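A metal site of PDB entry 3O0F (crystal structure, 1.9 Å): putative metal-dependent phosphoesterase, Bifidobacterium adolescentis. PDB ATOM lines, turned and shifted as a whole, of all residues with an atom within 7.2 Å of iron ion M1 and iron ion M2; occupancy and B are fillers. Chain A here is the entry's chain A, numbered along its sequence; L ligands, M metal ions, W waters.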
ATOM      1  N   HIS A  18     -13.545  28.917 -24.649  1.00  0.00           N
ATOM      2  CA  HIS A  18     -12.108  28.751 -24.480  1.00  0.00           C
ATOM      3  C   HIS A  18     -11.714  28.894 -22.998  1.00  0.00           C
ATOM      4  O   HIS A  18     -11.263  29.970 -22.576  1.00  0.00           O
ATOM      5  CB  HIS A  18     -11.427  29.821 -25.311  1.00  0.00           C
ATOM      6  CG  HIS A  18      -9.988  29.550 -25.585  1.00  0.00           C
ATOM      7  ND1 HIS A  18      -9.309  30.149 -26.636  1.00  0.00           N
ATOM      8  CD2 HIS A  18      -9.084  28.785 -24.928  1.00  0.00           C
ATOM      9  CE1 HIS A  18      -8.057  29.726 -26.631  1.00  0.00           C
ATOM     10  NE2 HIS A  18      -7.892  28.904 -25.606  1.00  0.00           N
ATOM     11  N   CYS A  19     -11.870  27.826 -22.221  1.00  0.00           N
ATOM     12  CA  CYS A  19     -11.671  27.864 -20.757  1.00  0.00           C
ATOM     13  C   CYS A  19     -10.842  26.643 -20.328  1.00  0.00           C
ATOM     14  O   CYS A  19     -11.120  25.523 -20.791  1.00  0.00           O
ATOM     15  CB  CYS A  19     -12.992  27.876 -20.016  1.00  0.00           C
ATOM     16  SG  CYS A  19     -14.141  29.154 -20.548  1.00  0.00           S
ATOM     17  N   HIS A  20      -9.820  26.881 -19.501  1.00  0.00           N
ATOM     18  CA  HIS A  20      -8.913  25.867 -18.987  1.00  0.00           C
ATOM     19  C   HIS A  20      -9.140  25.591 -17.494  1.00  0.00           C
ATOM     20  O   HIS A  20      -9.547  26.495 -16.755  1.00  0.00           O
ATOM     21  CB  HIS A  20      -7.474  26.316 -19.207  1.00  0.00           C
ATOM     22  CG  HIS A  20      -7.124  26.470 -20.648  1.00  0.00           C
ATOM     23  ND1 HIS A  20      -6.486  25.495 -21.358  1.00  0.00           N
ATOM     24  CD2 HIS A  20      -7.347  27.488 -21.522  1.00  0.00           C
ATOM     25  CE1 HIS A  20      -6.331  25.894 -22.611  1.00  0.00           C
ATOM     26  NE2 HIS A  20      -6.853  27.080 -22.736  1.00  0.00           N
ATOM     27  N   ASP A  25      -3.750  23.683 -17.327  1.00  0.00           N
ATOM     28  CA  ASP A  25      -3.070  24.782 -16.671  1.00  0.00           C
ATOM     29  C   ASP A  25      -3.968  25.842 -15.994  1.00  0.00           C
ATOM     30  O   ASP A  25      -3.486  26.910 -15.618  1.00  0.00           O
ATOM     31  CB  ASP A  25      -2.051  25.437 -17.609  1.00  0.00           C
ATOM     32  CG  ASP A  25      -2.651  25.991 -18.902  1.00  0.00           C
ATOM     33  OD1 ASP A  25      -3.854  25.755 -19.223  1.00  0.00           O
ATOM     34  OD2 ASP A  25      -1.875  26.697 -19.624  1.00  0.00           O
ATOM     35  N   ALA A  48     -11.822  23.345 -22.570  1.00  0.00           N
ATOM     36  CA  ALA A  48     -10.868  23.275 -23.699  1.00  0.00           C
ATOM     37  C   ALA A  48      -9.468  23.066 -23.195  1.00  0.00           C
ATOM     38  O   ALA A  48      -8.534  23.746 -23.644  1.00  0.00           O
ATOM     39  CB  ALA A  48     -10.934  24.562 -24.558  1.00  0.00           C
ATOM     40  N   HIS A  50      -5.662  21.661 -22.564  1.00  0.00           N
ATOM     41  CA  HIS A  50      -4.561  21.323 -23.489  1.00  0.00           C
ATOM     42  C   HIS A  50      -4.421  19.811 -23.632  1.00  0.00           C
ATOM     43  O   HIS A  50      -4.283  19.119 -22.639  1.00  0.00           O
ATOM     44  CB  HIS A  50      -3.244  21.874 -22.932  1.00  0.00           C
ATOM     45  CG  HIS A  50      -3.201  23.353 -22.860  1.00  0.00           C
ATOM     46  ND1 HIS A  50      -2.918  24.138 -23.958  1.00  0.00           N
ATOM     47  CD2 HIS A  50      -3.410  24.209 -21.826  1.00  0.00           C
ATOM     48  CE1 HIS A  50      -2.966  25.408 -23.609  1.00  0.00           C
ATOM     49  NE2 HIS A  50      -3.240  25.476 -22.328  1.00  0.00           N
ATOM     50  N   GLU A  75      -7.819  22.017 -26.421  1.00  0.00           N
ATOM     51  CA  GLU A  75      -6.903  22.893 -27.156  1.00  0.00           C
ATOM     52  C   GLU A  75      -5.679  22.055 -27.510  1.00  0.00           C
ATOM     53  O   GLU A  75      -4.961  21.552 -26.653  1.00  0.00           O
ATOM     54  CB  GLU A  75      -6.514  24.144 -26.351  1.00  0.00           C
ATOM     55  CG  GLU A  75      -5.584  24.998 -27.134  1.00  0.00           C
ATOM     56  CD  GLU A  75      -5.366  26.396 -26.545  1.00  0.00           C
ATOM     57  OE1 GLU A  75      -5.743  26.617 -25.435  1.00  0.00           O
ATOM     58  OE2 GLU A  75      -4.874  27.296 -27.275  1.00  0.00           O
ATOM     59  N   VAL A  85       1.037  26.868 -33.222  1.00  0.00           N
ATOM     60  CA  VAL A  85      -0.386  27.044 -33.504  1.00  0.00           C
ATOM     61  C   VAL A  85      -1.162  26.216 -32.478  1.00  0.00           C
ATOM     62  O   VAL A  85      -0.864  25.034 -32.264  1.00  0.00           O
ATOM     63  CB  VAL A  85      -0.780  26.522 -34.920  1.00  0.00           C
ATOM     64  CG1 VAL A  85      -2.275  26.755 -35.192  1.00  0.00           C
ATOM     65  CG2 VAL A  85       0.062  27.165 -36.033  1.00  0.00           C
ATOM     66  N   HIS A  86      -2.146  26.832 -31.850  1.00  0.00           N
ATOM     67  CA  HIS A  86      -3.070  26.132 -30.995  1.00  0.00           C
ATOM     68  C   HIS A  86      -4.406  25.998 -31.732  1.00  0.00           C
ATOM     69  O   HIS A  86      -4.913  26.964 -32.315  1.00  0.00           O
ATOM     70  CB  HIS A  86      -3.202  26.921 -29.676  1.00  0.00           C
ATOM     71  CG  HIS A  86      -1.996  26.795 -28.791  1.00  0.00           C
ATOM     72  ND1 HIS A  86      -1.998  27.172 -27.459  1.00  0.00           N
ATOM     73  CD2 HIS A  86      -0.755  26.289 -29.028  1.00  0.00           C
ATOM     74  CE1 HIS A  86      -0.810  26.928 -26.936  1.00  0.00           C
ATOM     75  NE2 HIS A  86      -0.043  26.393 -27.860  1.00  0.00           N
ATOM     76  N   MET A  87      -4.939  24.774 -31.712  1.00  0.00           N
ATOM     77  CA  MET A  87      -6.173  24.428 -32.412  1.00  0.00           C
ATOM     78  C   MET A  87      -7.204  24.043 -31.366  1.00  0.00           C
ATOM     79  O   MET A  87      -6.963  23.152 -30.571  1.00  0.00           O
ATOM     80  CB  MET A  87      -5.948  23.204 -33.277  1.00  0.00           C
ATOM     81  CG  MET A  87      -4.746  23.346 -34.218  1.00  0.00           C
ATOM     82  SD  MET A  87      -5.159  24.119 -35.932  1.00  0.00           S
ATOM     83  CE  MET A  87      -6.934  24.860 -35.705  1.00  0.00           C
ATOM     84  N   LEU A  88      -8.372  24.659 -31.435  1.00  0.00           N
ATOM     85  CA  LEU A  88      -9.493  24.290 -30.581  1.00  0.00           C
ATOM     86  C   LEU A  88     -10.319  23.243 -31.352  1.00  0.00           C
ATOM     87  O   LEU A  88     -10.642  23.458 -32.522  1.00  0.00           O
ATOM     88  CB  LEU A  88     -10.332  25.547 -30.302  1.00  0.00           C
ATOM     89  CG  LEU A  88      -9.719  26.649 -29.442  1.00  0.00           C
ATOM     90  CD1 LEU A  88     -10.603  27.880 -29.523  1.00  0.00           C
ATOM     91  CD2 LEU A  88      -9.536  26.258 -27.982  1.00  0.00           C
ATOM     92  N   ALA A 202      -6.967  28.863 -32.895  1.00  0.00           N
ATOM     93  CA  ALA A 202      -7.010  29.702 -31.679  1.00  0.00           C
ATOM     94  C   ALA A 202      -6.069  30.935 -31.800  1.00  0.00           C
ATOM     95  O   ALA A 202      -5.000  30.830 -32.375  1.00  0.00           O
ATOM     96  CB  ALA A 202      -6.619  28.887 -30.445  1.00  0.00           C
ATOM     97  N   HIS A 203      -6.544  32.073 -31.292  1.00  0.00           N
ATOM     98  CA  HIS A 203      -5.829  33.389 -31.234  1.00  0.00           C
ATOM     99  C   HIS A 203      -4.762  33.545 -32.362  1.00  0.00           C
ATOM    100  O   HIS A 203      -3.566  33.713 -32.084  1.00  0.00           O
ATOM    101  CB  HIS A 203      -5.210  33.569 -29.823  1.00  0.00           C
ATOM    102  CG  HIS A 203      -4.493  32.355 -29.307  1.00  0.00           C
ATOM    103  ND1 HIS A 203      -3.312  31.890 -29.857  1.00  0.00           N
ATOM    104  CD2 HIS A 203      -4.797  31.491 -28.295  1.00  0.00           C
ATOM    105  CE1 HIS A 203      -2.920  30.793 -29.225  1.00  0.00           C
ATOM    106  NE2 HIS A 203      -3.805  30.531 -28.275  1.00  0.00           N
ATOM    107  N   ASP A 206      -2.123  36.568 -32.633  1.00  0.00           N
ATOM    108  CA  ASP A 206      -1.448  36.923 -31.378  1.00  0.00           C
ATOM    109  C   ASP A 206       0.100  36.862 -31.530  1.00  0.00           C
ATOM    110  O   ASP A 206       0.653  35.797 -31.725  1.00  0.00           O
ATOM    111  CB  ASP A 206      -1.970  36.013 -30.246  1.00  0.00           C
ATOM    112  CG  ASP A 206      -1.404  36.349 -28.890  1.00  0.00           C
ATOM    113  OD1 ASP A 206      -0.583  37.288 -28.747  1.00  0.00           O
ATOM    114  OD2 ASP A 206      -1.806  35.662 -27.922  1.00  0.00           O
ATOM    115  N   GLU A 231     -10.824  31.835 -34.278  1.00  0.00           N
ATOM    116  CA  GLU A 231     -11.094  32.535 -33.052  1.00  0.00           C
ATOM    117  C   GLU A 231     -10.654  33.966 -33.265  1.00  0.00           C
ATOM    118  O   GLU A 231      -9.452  34.227 -33.412  1.00  0.00           O
ATOM    119  CB  GLU A 231     -10.310  31.890 -31.903  1.00  0.00           C
ATOM    120  CG  GLU A 231     -10.448  32.630 -30.614  1.00  0.00           C
ATOM    121  CD  GLU A 231      -9.777  31.904 -29.457  1.00  0.00           C
ATOM    122  OE1 GLU A 231      -8.533  31.698 -29.530  1.00  0.00           O
ATOM    123  OE2 GLU A 231     -10.474  31.548 -28.478  1.00  0.00           O
ATOM    124  N   HIS A 234     -10.684  37.613 -29.018  1.00  0.00           N
ATOM    125  CA  HIS A 234      -9.710  37.106 -28.060  1.00  0.00           C
ATOM    126  C   HIS A 234      -8.778  38.255 -27.733  1.00  0.00           C
ATOM    127  O   HIS A 234      -8.392  39.015 -28.612  1.00  0.00           O
ATOM    128  CB  HIS A 234      -8.933  35.936 -28.652  1.00  0.00           C
ATOM    129  CG  HIS A 234      -7.982  35.262 -27.705  1.00  0.00           C
ATOM    130  ND1 HIS A 234      -6.746  35.775 -27.392  1.00  0.00           N
ATOM    131  CD2 HIS A 234      -8.066  34.066 -27.056  1.00  0.00           C
ATOM    132  CE1 HIS A 234      -6.133  34.966 -26.544  1.00  0.00           C
ATOM    133  NE2 HIS A 234      -6.896  33.914 -26.336  1.00  0.00           N
ATOM    134  N   SER A 260     -12.422  33.545 -23.633  1.00  0.00           N
ATOM    135  CA  SER A 260     -11.621  34.296 -22.673  1.00  0.00           C
ATOM    136  C   SER A 260     -10.201  33.783 -22.532  1.00  0.00           C
ATOM    137  O   SER A 260      -9.323  34.553 -22.184  1.00  0.00           O
ATOM    138  CB  SER A 260     -12.260  34.258 -21.306  1.00  0.00           C
ATOM    139  OG  SER A 260     -12.359  32.917 -20.839  1.00  0.00           O
ATOM    140  N   ASP A 261      -9.971  32.496 -22.824  1.00  0.00           N
ATOM    141  CA  ASP A 261      -8.740  31.835 -22.423  1.00  0.00           C
ATOM    142  C   ASP A 261      -8.576  31.914 -20.894  1.00  0.00           C
ATOM    143  O   ASP A 261      -7.481  32.076 -20.400  1.00  0.00           O
ATOM    144  CB  ASP A 261      -7.538  32.476 -23.108  1.00  0.00           C
ATOM    145  CG  ASP A 261      -6.619  31.471 -23.694  1.00  0.00           C
ATOM    146  OD1 ASP A 261      -6.599  30.346 -23.177  1.00  0.00           O
ATOM    147  OD2 ASP A 261      -5.963  31.817 -24.691  1.00  0.00           O
ATOM    148  N   TRP A 262      -9.678  31.801 -20.175  1.00  0.00           N
ATOM    149  CA  TRP A 262      -9.642  31.764 -18.737  1.00  0.00           C
ATOM    150  C   TRP A 262      -8.808  30.598 -18.246  1.00  0.00           C
ATOM    151  O   TRP A 262      -8.943  29.457 -18.721  1.00  0.00           O
ATOM    152  CB  TRP A 262     -11.056  31.631 -18.230  1.00  0.00           C
ATOM    153  CG  TRP A 262     -11.310  31.606 -16.764  1.00  0.00           C
ATOM    154  CD1 TRP A 262     -11.371  32.668 -15.943  1.00  0.00           C
ATOM    155  CD2 TRP A 262     -11.702  30.463 -15.994  1.00  0.00           C
ATOM    156  NE1 TRP A 262     -11.736  32.267 -14.674  1.00  0.00           N
ATOM    157  CE2 TRP A 262     -12.000  30.921 -14.702  1.00  0.00           C
ATOM    158  CE3 TRP A 262     -11.843  29.096 -16.288  1.00  0.00           C
ATOM    159  CZ2 TRP A 262     -12.371  30.057 -13.692  1.00  0.00           C
ATOM    160  CZ3 TRP A 262     -12.237  28.233 -15.285  1.00  0.00           C
ATOM    161  CH2 TRP A 262     -12.497  28.730 -14.000  1.00  0.00           C
ATOM    162  N   HIS A 263      -7.977  30.906 -17.257  1.00  0.00           N
ATOM    163  CA  HIS A 263      -7.219  29.910 -16.537  1.00  0.00           C
ATOM    164  C   HIS A 263      -7.407  30.140 -15.038  1.00  0.00           C
ATOM    165  O   HIS A 263      -6.539  29.795 -14.228  1.00  0.00           O
ATOM    166  CB  HIS A 263      -5.727  30.060 -16.875  1.00  0.00           C
ATOM    167  CG  HIS A 263      -5.342  29.640 -18.253  1.00  0.00           C
ATOM    168  ND1 HIS A 263      -5.775  30.273 -19.407  1.00  0.00           N
ATOM    169  CD2 HIS A 263      -4.507  28.662 -18.670  1.00  0.00           C
ATOM    170  CE1 HIS A 263      -5.232  29.696 -20.456  1.00  0.00           C
ATOM    171  NE2 HIS A 263      -4.450  28.721 -20.032  1.00  0.00           N
ATOM    172  N   LYS A 267      -4.073  33.435 -14.927  1.00  0.00           N
ATOM    173  CA  LYS A 267      -3.924  34.520 -15.875  1.00  0.00           C
ATOM    174  C   LYS A 267      -4.864  35.639 -15.468  1.00  0.00           C
ATOM    175  O   LYS A 267      -5.804  35.415 -14.750  1.00  0.00           O
ATOM    176  CB  LYS A 267      -4.306  34.048 -17.292  1.00  0.00           C
ATOM    177  CG  LYS A 267      -3.265  33.260 -18.076  1.00  0.00           C
ATOM    178  CD  LYS A 267      -3.727  33.121 -19.517  1.00  0.00           C
ATOM    179  CE  LYS A 267      -2.814  32.298 -20.406  1.00  0.00           C
ATOM    180  NZ  LYS A 267      -3.387  32.326 -21.779  1.00  0.00           N
HETATM  181  P1  LIG L   1      -2.976  28.982 -23.379  1.00  0.00           P
HETATM  182  O1  LIG L   1      -2.727  30.470 -23.197  1.00  0.00           O
HETATM  183  O2  LIG L   1      -2.365  28.592 -24.707  1.00  0.00           O
HETATM  184  O3  LIG L   1      -2.570  28.148 -22.140  1.00  0.00           O
HETATM  185  O4  LIG L   1      -4.423  28.648 -23.382  1.00  0.00           O
HETATM  186  P1  LG2 L   2       3.978  25.198 -22.936  1.00  0.00           P
HETATM  187  O1  LG2 L   2       2.935  24.732 -23.900  1.00  0.00           O
HETATM  188  O2  LG2 L   2       4.255  24.112 -21.928  1.00  0.00           O
HETATM  189  O3  LG2 L   2       5.230  25.788 -23.586  1.00  0.00           O
HETATM  190  O4  LG2 L   2       3.308  26.394 -22.104  1.00  0.00           O
HETATM  191  C1  LG2 L   2       2.992  27.612 -22.741  1.00  0.00           C
HETATM  192  C2  LG2 L   2       1.580  27.944 -22.365  1.00  0.00           C
HETATM  193  O5  LG2 L   2       1.477  28.492 -21.026  1.00  0.00           O
HETATM  194  C3  LG2 L   2       0.995  28.970 -23.326  1.00  0.00           C
HETATM  195  O6  LG2 L   2       0.054  28.326 -24.175  1.00  0.00           O
HETATM  196  C4  LG2 L   2       0.281  29.860 -22.326  1.00  0.00           C
HETATM  197  O7  LG2 L   2      -0.517  30.988 -22.675  1.00  0.00           O
HETATM  198  C5  LG2 L   2       0.208  29.129 -20.986  1.00  0.00           C
HETATM  199  N1  LG2 L   2       0.028  30.045 -19.840  1.00  0.00           N
HETATM  200  C6  LG2 L   2      -0.761  29.801 -18.795  1.00  0.00           C
HETATM  201  N2  LG2 L   2      -0.693  30.826 -17.915  1.00  0.00           N
HETATM  202  C7  LG2 L   2       0.151  31.746 -18.406  1.00  0.00           C
HETATM  203  C8  LG2 L   2       0.655  33.064 -17.982  1.00  0.00           C
HETATM  204  N3  LG2 L   2       0.250  33.634 -16.798  1.00  0.00           N
HETATM  205  N4  LG2 L   2       1.542  33.662 -18.792  1.00  0.00           N
HETATM  206  C9  LG2 L   2       1.970  33.135 -19.960  1.00  0.00           C
HETATM  207  N5  LG2 L   2       1.543  31.951 -20.407  1.00  0.00           N
HETATM  208  C10 LG2 L   2       0.638  31.228 -19.683  1.00  0.00           C
HETATM  209 FE    FE M   1      -3.548  28.880 -26.702  1.00  0.00          FE
HETATM  210 FE    FE M   2      -6.091  28.478 -24.394  1.00  0.00          FE
HETATM  211 ZN    ZN M   3      -3.541  27.159 -21.061  1.00  0.00          ZN
HETATM  212  O   HOH W   1      -1.782  31.622 -25.772  1.00  0.00           O
HETATM  213  O   HOH W   2      -5.118  29.710 -25.762  1.00  0.00           O
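The side-chain amino group (NZ) of Lys 267 is in hydrogen-bond range of an oxygen (O7) of LG2 L2 (3.3 Å).
OE2 of Glu 231 sits at hydrogen-bond distance from ND1 of His 18, 2.6 Å away.
A ring nitrogen (ND1) of His 20 sits close to a ring nitrogen (NE2) of His 50 (3.4 Å).
The backbone carbonyl oxygen (O) of Asp 261 lies within hydrogen-bond range of a ring nitrogen (ND1) of His 263, 2.7 Å away.
The backbone carbonyl oxygen of His 86 lies within hydrogen-bond range of the backbone NH of Ala 202, 2.9 Å away.
N of His 203 is in hydrogen-bond range of OE1 of Glu 231, 2.7 Å away.
The backbone carbonyl oxygen of His 18 is in hydrogen-bond range of the backbone NH of Trp 262 (3.4 Å).
The side-chain carboxylate (OD2) of Asp 261 lies within salt-bridge range of the side-chain amino group (NZ) of Lys 267 (3.9 Å).
ND1 of His 20 sits close to OD1 of Asp 25 (3.4 Å).
Of the 21 residues printed, 3 come within 4 Å of iron ion M1.
Of the 21 residues printed, 4 come within 4 Å of iron ion M2.
Iron ion M1 is bound by water W2 (2.0 Å), the side-chain carboxylate of Glu 75 (2.1 Å), a ring nitrogen (NE2) of His 203 (2.3 Å), an oxygen (O2) of LIG L1 (2.3 Å) and a ring nitrogen (ND1) of His 86 (2.4 Å).
Iron ion M2 is bound by O4 of LIG L1 (2.0 Å), water W2 (2.1 Å), OE1 of Glu 75 (2.2 Å), NE2 of His 18 (2.2 Å), OD1 of Asp 261 (2.3 Å) and NE2 of His 20 (2.3 Å).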
